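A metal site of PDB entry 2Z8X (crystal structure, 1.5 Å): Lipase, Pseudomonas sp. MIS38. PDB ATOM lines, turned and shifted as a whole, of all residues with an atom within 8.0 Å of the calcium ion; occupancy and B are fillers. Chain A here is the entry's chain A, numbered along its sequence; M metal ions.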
ATOM      1  N   THR A 369     -27.239   8.100 -10.404  1.00  0.00           N
ATOM      2  CA  THR A 369     -28.077   8.610  -9.320  1.00  0.00           C
ATOM      3  C   THR A 369     -28.007  10.127  -9.295  1.00  0.00           C
ATOM      4  O   THR A 369     -26.921  10.705  -9.424  1.00  0.00           O
ATOM      5  CB  THR A 369     -27.628   8.025  -7.960  1.00  0.00           C
ATOM      6  OG1 THR A 369     -27.633   6.588  -8.052  1.00  0.00           O
ATOM      7  CG2 THR A 369     -28.561   8.448  -6.838  1.00  0.00           C
ATOM      8  N   GLN A 381     -24.151  13.050   0.081  1.00  0.00           N
ATOM      9  CA  GLN A 381     -23.243  11.909  -0.084  1.00  0.00           C
ATOM     10  C   GLN A 381     -23.600  11.071  -1.322  1.00  0.00           C
ATOM     11  O   GLN A 381     -24.646  10.411  -1.362  1.00  0.00           O
ATOM     12  CB  GLN A 381     -23.257  11.039   1.186  1.00  0.00           C
ATOM     13  CG  GLN A 381     -22.608   9.664   1.076  1.00  0.00           C
ATOM     14  CD  GLN A 381     -21.105   9.667   1.272  1.00  0.00           C
ATOM     15  OE1 GLN A 381     -20.603   9.947   2.367  1.00  0.00           O
ATOM     16  NE2 GLN A 381     -20.373   9.329   0.217  1.00  0.00           N
ATOM     17  N   GLY A 382     -22.718  11.089  -2.313  1.00  0.00           N
ATOM     18  CA  GLY A 382     -22.894  10.218  -3.468  1.00  0.00           C
ATOM     19  C   GLY A 382     -22.284   8.842  -3.236  1.00  0.00           C
ATOM     20  O   GLY A 382     -21.391   8.681  -2.390  1.00  0.00           O
ATOM     21  N   GLY A 383     -22.772   7.856  -3.974  1.00  0.00           N
ATOM     22  CA  GLY A 383     -22.334   6.470  -3.811  1.00  0.00           C
ATOM     23  C   GLY A 383     -21.096   6.146  -4.627  1.00  0.00           C
ATOM     24  O   GLY A 383     -20.472   7.037  -5.216  1.00  0.00           O
ATOM     25  N   SER A 384     -20.753   4.862  -4.670  1.00  0.00           N
ATOM     26  CA  SER A 384     -19.558   4.387  -5.356  1.00  0.00           C
ATOM     27  C   SER A 384     -19.770   4.227  -6.869  1.00  0.00           C
ATOM     28  O   SER A 384     -18.814   4.020  -7.611  1.00  0.00           O
ATOM     29  CB  SER A 384     -19.070   3.074  -4.740  1.00  0.00           C
ATOM     30  OG  SER A 384     -20.036   2.060  -4.916  1.00  0.00           O
ATOM     31  N   GLY A 385     -21.021   4.334  -7.303  1.00  0.00           N
ATOM     32  CA  GLY A 385     -21.345   4.397  -8.723  1.00  0.00           C
ATOM     33  C   GLY A 385     -21.292   5.826  -9.210  1.00  0.00           C
ATOM     34  O   GLY A 385     -20.605   6.686  -8.624  1.00  0.00           O
ATOM     35  N   ASN A 386     -22.038   6.103 -10.272  1.00  0.00           N
ATOM     36  CA  ASN A 386     -22.002   7.400 -10.946  1.00  0.00           C
ATOM     37  C   ASN A 386     -23.107   8.317 -10.449  1.00  0.00           C
ATOM     38  O   ASN A 386     -24.266   7.903 -10.389  1.00  0.00           O
ATOM     39  CB  ASN A 386     -22.091   7.191 -12.462  1.00  0.00           C
ATOM     40  CG  ASN A 386     -21.052   6.206 -12.966  1.00  0.00           C
ATOM     41  OD1 ASN A 386     -19.893   6.225 -12.520  1.00  0.00           O
ATOM     42  ND2 ASN A 386     -21.449   5.343 -13.883  1.00  0.00           N
ATOM     43  N   ASP A 387     -22.739   9.538 -10.058  1.00  0.00           N
ATOM     44  CA  ASP A 387     -23.636  10.462  -9.354  1.00  0.00           C
ATOM     45  C   ASP A 387     -23.635  11.850  -9.942  1.00  0.00           C
ATOM     46  O   ASP A 387     -22.606  12.363 -10.390  1.00  0.00           O
ATOM     47  CB  ASP A 387     -23.251  10.589  -7.866  1.00  0.00           C
ATOM     48  CG  ASP A 387     -23.411   9.300  -7.099  1.00  0.00           C
ATOM     49  OD1 ASP A 387     -24.433   9.157  -6.400  1.00  0.00           O
ATOM     50  OD2 ASP A 387     -22.505   8.435  -7.205  1.00  0.00           O
ATOM     51  N   TYR A 388     -24.803  12.485  -9.854  1.00  0.00           N
ATOM     52  CA  TYR A 388     -25.006  13.872 -10.237  1.00  0.00           C
ATOM     53  C   TYR A 388     -25.541  14.568  -8.998  1.00  0.00           C
ATOM     54  O   TYR A 388     -26.686  14.373  -8.623  1.00  0.00           O
ATOM     55  CB  TYR A 388     -25.975  13.960 -11.411  1.00  0.00           C
ATOM     56  CG  TYR A 388     -25.451  13.278 -12.648  1.00  0.00           C
ATOM     57  CD1 TYR A 388     -24.632  13.963 -13.545  1.00  0.00           C
ATOM     58  CD2 TYR A 388     -25.765  11.944 -12.923  1.00  0.00           C
ATOM     59  CE1 TYR A 388     -24.144  13.332 -14.686  1.00  0.00           C
ATOM     60  CE2 TYR A 388     -25.275  11.301 -14.071  1.00  0.00           C
ATOM     61  CZ  TYR A 388     -24.462  12.012 -14.932  1.00  0.00           C
ATOM     62  OH  TYR A 388     -23.972  11.412 -16.068  1.00  0.00           O
ATOM     63  N   LEU A 389     -24.684  15.362  -8.361  1.00  0.00           N
ATOM     64  CA  LEU A 389     -24.994  15.961  -7.056  1.00  0.00           C
ATOM     65  C   LEU A 389     -25.196  17.458  -7.210  1.00  0.00           C
ATOM     66  O   LEU A 389     -24.319  18.153  -7.728  1.00  0.00           O
ATOM     67  CB  LEU A 389     -23.831  15.690  -6.081  1.00  0.00           C
ATOM     68  CG  LEU A 389     -23.373  14.232  -5.971  1.00  0.00           C
ATOM     69  CD1 LEU A 389     -22.195  14.115  -4.979  1.00  0.00           C
ATOM     70  CD2 LEU A 389     -24.513  13.337  -5.560  1.00  0.00           C
ATOM     71  N   ARG A 399     -19.776  14.592  -0.263  1.00  0.00           N
ATOM     72  CA  ARG A 399     -18.876  13.445  -0.220  1.00  0.00           C
ATOM     73  C   ARG A 399     -19.299  12.560  -1.379  1.00  0.00           C
ATOM     74  O   ARG A 399     -20.444  12.660  -1.835  1.00  0.00           O
ATOM     75  CB  ARG A 399     -19.026  12.674   1.090  1.00  0.00           C
ATOM     76  CG  ARG A 399     -18.364  13.361   2.266  1.00  0.00           C
ATOM     77  CD  ARG A 399     -18.714  12.654   3.555  1.00  0.00           C
ATOM     78  NE  ARG A 399     -17.892  13.170   4.651  1.00  0.00           N
ATOM     79  CZ  ARG A 399     -18.008  12.777   5.910  1.00  0.00           C
ATOM     80  NH1 ARG A 399     -18.925  11.875   6.259  1.00  0.00           N
ATOM     81  NH2 ARG A 399     -17.214  13.300   6.836  1.00  0.00           N
ATOM     82  N   ASP A 400     -18.397  11.723  -1.867  1.00  0.00           N
ATOM     83  CA  ASP A 400     -18.786  10.763  -2.884  1.00  0.00           C
ATOM     84  C   ASP A 400     -17.881   9.553  -2.847  1.00  0.00           C
ATOM     85  O   ASP A 400     -16.669   9.682  -2.679  1.00  0.00           O
ATOM     86  CB  ASP A 400     -18.769  11.411  -4.284  1.00  0.00           C
ATOM     87  CG  ASP A 400     -19.250  10.458  -5.341  1.00  0.00           C
ATOM     88  OD1 ASP A 400     -20.464  10.449  -5.633  1.00  0.00           O
ATOM     89  OD2 ASP A 400     -18.437   9.668  -5.866  1.00  0.00           O
ATOM     90  N   GLY A 401     -18.474   8.379  -3.023  1.00  0.00           N
ATOM     91  CA  GLY A 401     -17.767   7.108  -2.846  1.00  0.00           C
ATOM     92  C   GLY A 401     -16.963   6.564  -4.021  1.00  0.00           C
ATOM     93  O   GLY A 401     -16.351   5.504  -3.902  1.00  0.00           O
ATOM     94  N   GLY A 402     -16.961   7.268  -5.140  1.00  0.00           N
ATOM     95  CA  GLY A 402     -16.195   6.837  -6.317  1.00  0.00           C
ATOM     96  C   GLY A 402     -16.968   6.968  -7.615  1.00  0.00           C
ATOM     97  O   GLY A 402     -18.022   7.610  -7.676  1.00  0.00           O
ATOM     98  N   GLY A 403     -16.446   6.349  -8.670  1.00  0.00           N
ATOM     99  CA  GLY A 403     -17.076   6.415  -9.967  1.00  0.00           C
ATOM    100  C   GLY A 403     -16.897   7.747 -10.676  1.00  0.00           C
ATOM    101  O   GLY A 403     -15.946   8.497 -10.408  1.00  0.00           O
ATOM    102  N   TYR A 404     -17.828   8.024 -11.583  1.00  0.00           N
ATOM    103  CA  TYR A 404     -17.790   9.217 -12.429  1.00  0.00           C
ATOM    104  C   TYR A 404     -18.978  10.106 -12.076  1.00  0.00           C
ATOM    105  O   TYR A 404     -20.122   9.633 -12.039  1.00  0.00           O
ATOM    106  CB  TYR A 404     -17.798   8.827 -13.913  1.00  0.00           C
ATOM    107  CG  TYR A 404     -16.616   7.950 -14.273  1.00  0.00           C
ATOM    108  CD1 TYR A 404     -15.465   8.505 -14.816  1.00  0.00           C
ATOM    109  CD2 TYR A 404     -16.631   6.578 -14.013  1.00  0.00           C
ATOM    110  CE1 TYR A 404     -14.356   7.703 -15.129  1.00  0.00           C
ATOM    111  CE2 TYR A 404     -15.531   5.779 -14.308  1.00  0.00           C
ATOM    112  CZ  TYR A 404     -14.404   6.349 -14.868  1.00  0.00           C
ATOM    113  OH  TYR A 404     -13.319   5.563 -15.175  1.00  0.00           O
ATOM    114  N   ASN A 405     -18.679  11.363 -11.777  1.00  0.00           N
ATOM    115  CA  ASN A 405     -19.667  12.247 -11.149  1.00  0.00           C
ATOM    116  C   ASN A 405     -19.642  13.655 -11.693  1.00  0.00           C
ATOM    117  O   ASN A 405     -18.614  14.113 -12.175  1.00  0.00           O
ATOM    118  CB  ASN A 405     -19.412  12.336  -9.630  1.00  0.00           C
ATOM    119  CG  ASN A 405     -19.081  10.998  -9.013  1.00  0.00           C
ATOM    120  OD1 ASN A 405     -19.950  10.139  -8.812  1.00  0.00           O
ATOM    121  ND2 ASN A 405     -17.797  10.796  -8.700  1.00  0.00           N
ATOM    122  N   VAL A 406     -20.771  14.347 -11.575  1.00  0.00           N
ATOM    123  CA  VAL A 406     -20.786  15.798 -11.742  1.00  0.00           C
ATOM    124  C   VAL A 406     -21.292  16.361 -10.431  1.00  0.00           C
ATOM    125  O   VAL A 406     -22.296  15.884  -9.897  1.00  0.00           O
ATOM    126  CB  VAL A 406     -21.673  16.269 -12.930  1.00  0.00           C
ATOM    127  CG1 VAL A 406     -21.625  17.782 -13.067  1.00  0.00           C
ATOM    128  CG2 VAL A 406     -21.224  15.597 -14.234  1.00  0.00           C
ATOM    129  N   ILE A 407     -20.575  17.344  -9.882  1.00  0.00           N
ATOM    130  CA  ILE A 407     -20.925  17.919  -8.594  1.00  0.00           C
ATOM    131  C   ILE A 407     -21.054  19.418  -8.754  1.00  0.00           C
ATOM    132  O   ILE A 407     -20.074  20.105  -9.050  1.00  0.00           O
ATOM    133  CB  ILE A 407     -19.854  17.578  -7.523  1.00  0.00           C
ATOM    134  CG1 ILE A 407     -19.621  16.062  -7.465  1.00  0.00           C
ATOM    135  CG2 ILE A 407     -20.314  18.094  -6.164  1.00  0.00           C
ATOM    136  CD1 ILE A 407     -18.533  15.601  -6.496  1.00  0.00           C
ATOM    137  N   ASP A 439      -9.733  10.158  -8.988  1.00  0.00           N
ATOM    138  CA  ASP A 439      -9.330   9.318  -7.858  1.00  0.00           C
ATOM    139  C   ASP A 439      -8.292   8.271  -8.278  1.00  0.00           C
ATOM    140  O   ASP A 439      -7.962   8.168  -9.461  1.00  0.00           O
ATOM    141  CB  ASP A 439     -10.554   8.720  -7.123  1.00  0.00           C
ATOM    142  CG  ASP A 439     -11.314   7.683  -7.951  1.00  0.00           C
ATOM    143  OD1 ASP A 439     -10.705   6.959  -8.768  1.00  0.00           O
ATOM    144  OD2 ASP A 439     -12.549   7.573  -7.739  1.00  0.00           O
ATOM    145  N   ILE A 444     -13.550  10.042 -12.367  1.00  0.00           N
ATOM    146  CA  ILE A 444     -13.462  11.480 -12.533  1.00  0.00           C
ATOM    147  C   ILE A 444     -14.748  12.155 -12.076  1.00  0.00           C
ATOM    148  O   ILE A 444     -15.847  11.745 -12.474  1.00  0.00           O
ATOM    149  CB  ILE A 444     -13.168  11.890 -13.990  1.00  0.00           C
ATOM    150  CG1 ILE A 444     -11.784  11.389 -14.448  1.00  0.00           C
ATOM    151  CG2 ILE A 444     -13.233  13.406 -14.155  1.00  0.00           C
ATOM    152  CD1 ILE A 444     -11.563  11.508 -15.979  1.00  0.00           C
ATOM    153  N   SER A 445     -14.600  13.172 -11.229  1.00  0.00           N
ATOM    154  CA  SER A 445     -15.693  14.104 -10.928  1.00  0.00           C
ATOM    155  C   SER A 445     -15.438  15.432 -11.606  1.00  0.00           C
ATOM    156  O   SER A 445     -14.352  16.013 -11.455  1.00  0.00           O
ATOM    157  CB  SER A 445     -15.817  14.342  -9.420  1.00  0.00           C
ATOM    158  OG  SER A 445     -16.101  13.137  -8.718  1.00  0.00           O
HETATM  159 CA    CA M   1     -20.150   8.432  -7.123  1.00  0.00          CA
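The backbone NH (N) of Asp 387 lies within hydrogen-bond range of the backbone carbonyl oxygen (O) of Tyr 404, at 3.3 Å. The backbone NH (N) of Val 406 is in hydrogen-bond range of the backbone carbonyl oxygen (O) of Asp 387 (3.0 Å). N of Gly 401 lies close to O of Gly 383 (3.3 Å). The backbone carbonyl oxygen of Gly 403 is in hydrogen-bond range of the side-chain amide nitrogen of Asn 405, 3.4 Å away. The side-chain hydroxyl (OG) of Ser 445 lies within hydrogen-bond range of the side-chain amide nitrogen (ND2) of Asn 405. O of Ile 444 is in hydrogen-bond range of N of Asn 405 (2.9 Å).
Within 4 Å of the calcium ion: Gly 383, Gly 385, Asp 387, Asp 400, Gly 402 and Asn 405.
The backbone carbonyl oxygen (O) of Gly 402 binds the calcium ion, 2.3 Å away. O of Gly 385 is bound to the calcium ion (2.3 Å). OD2 of Asp 387 binds the calcium ion. The calcium ion is bound by the backbone carbonyl oxygen (O) of Gly 383, at 2.4 Å. OD1 of Asn 405 is bound to the calcium ion (2.4 Å). OD2 of Asp 400 is bound to the calcium ion (2.5 Å). The calcium ion is bound by the side-chain carboxylate (OD1) of Asp 400.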
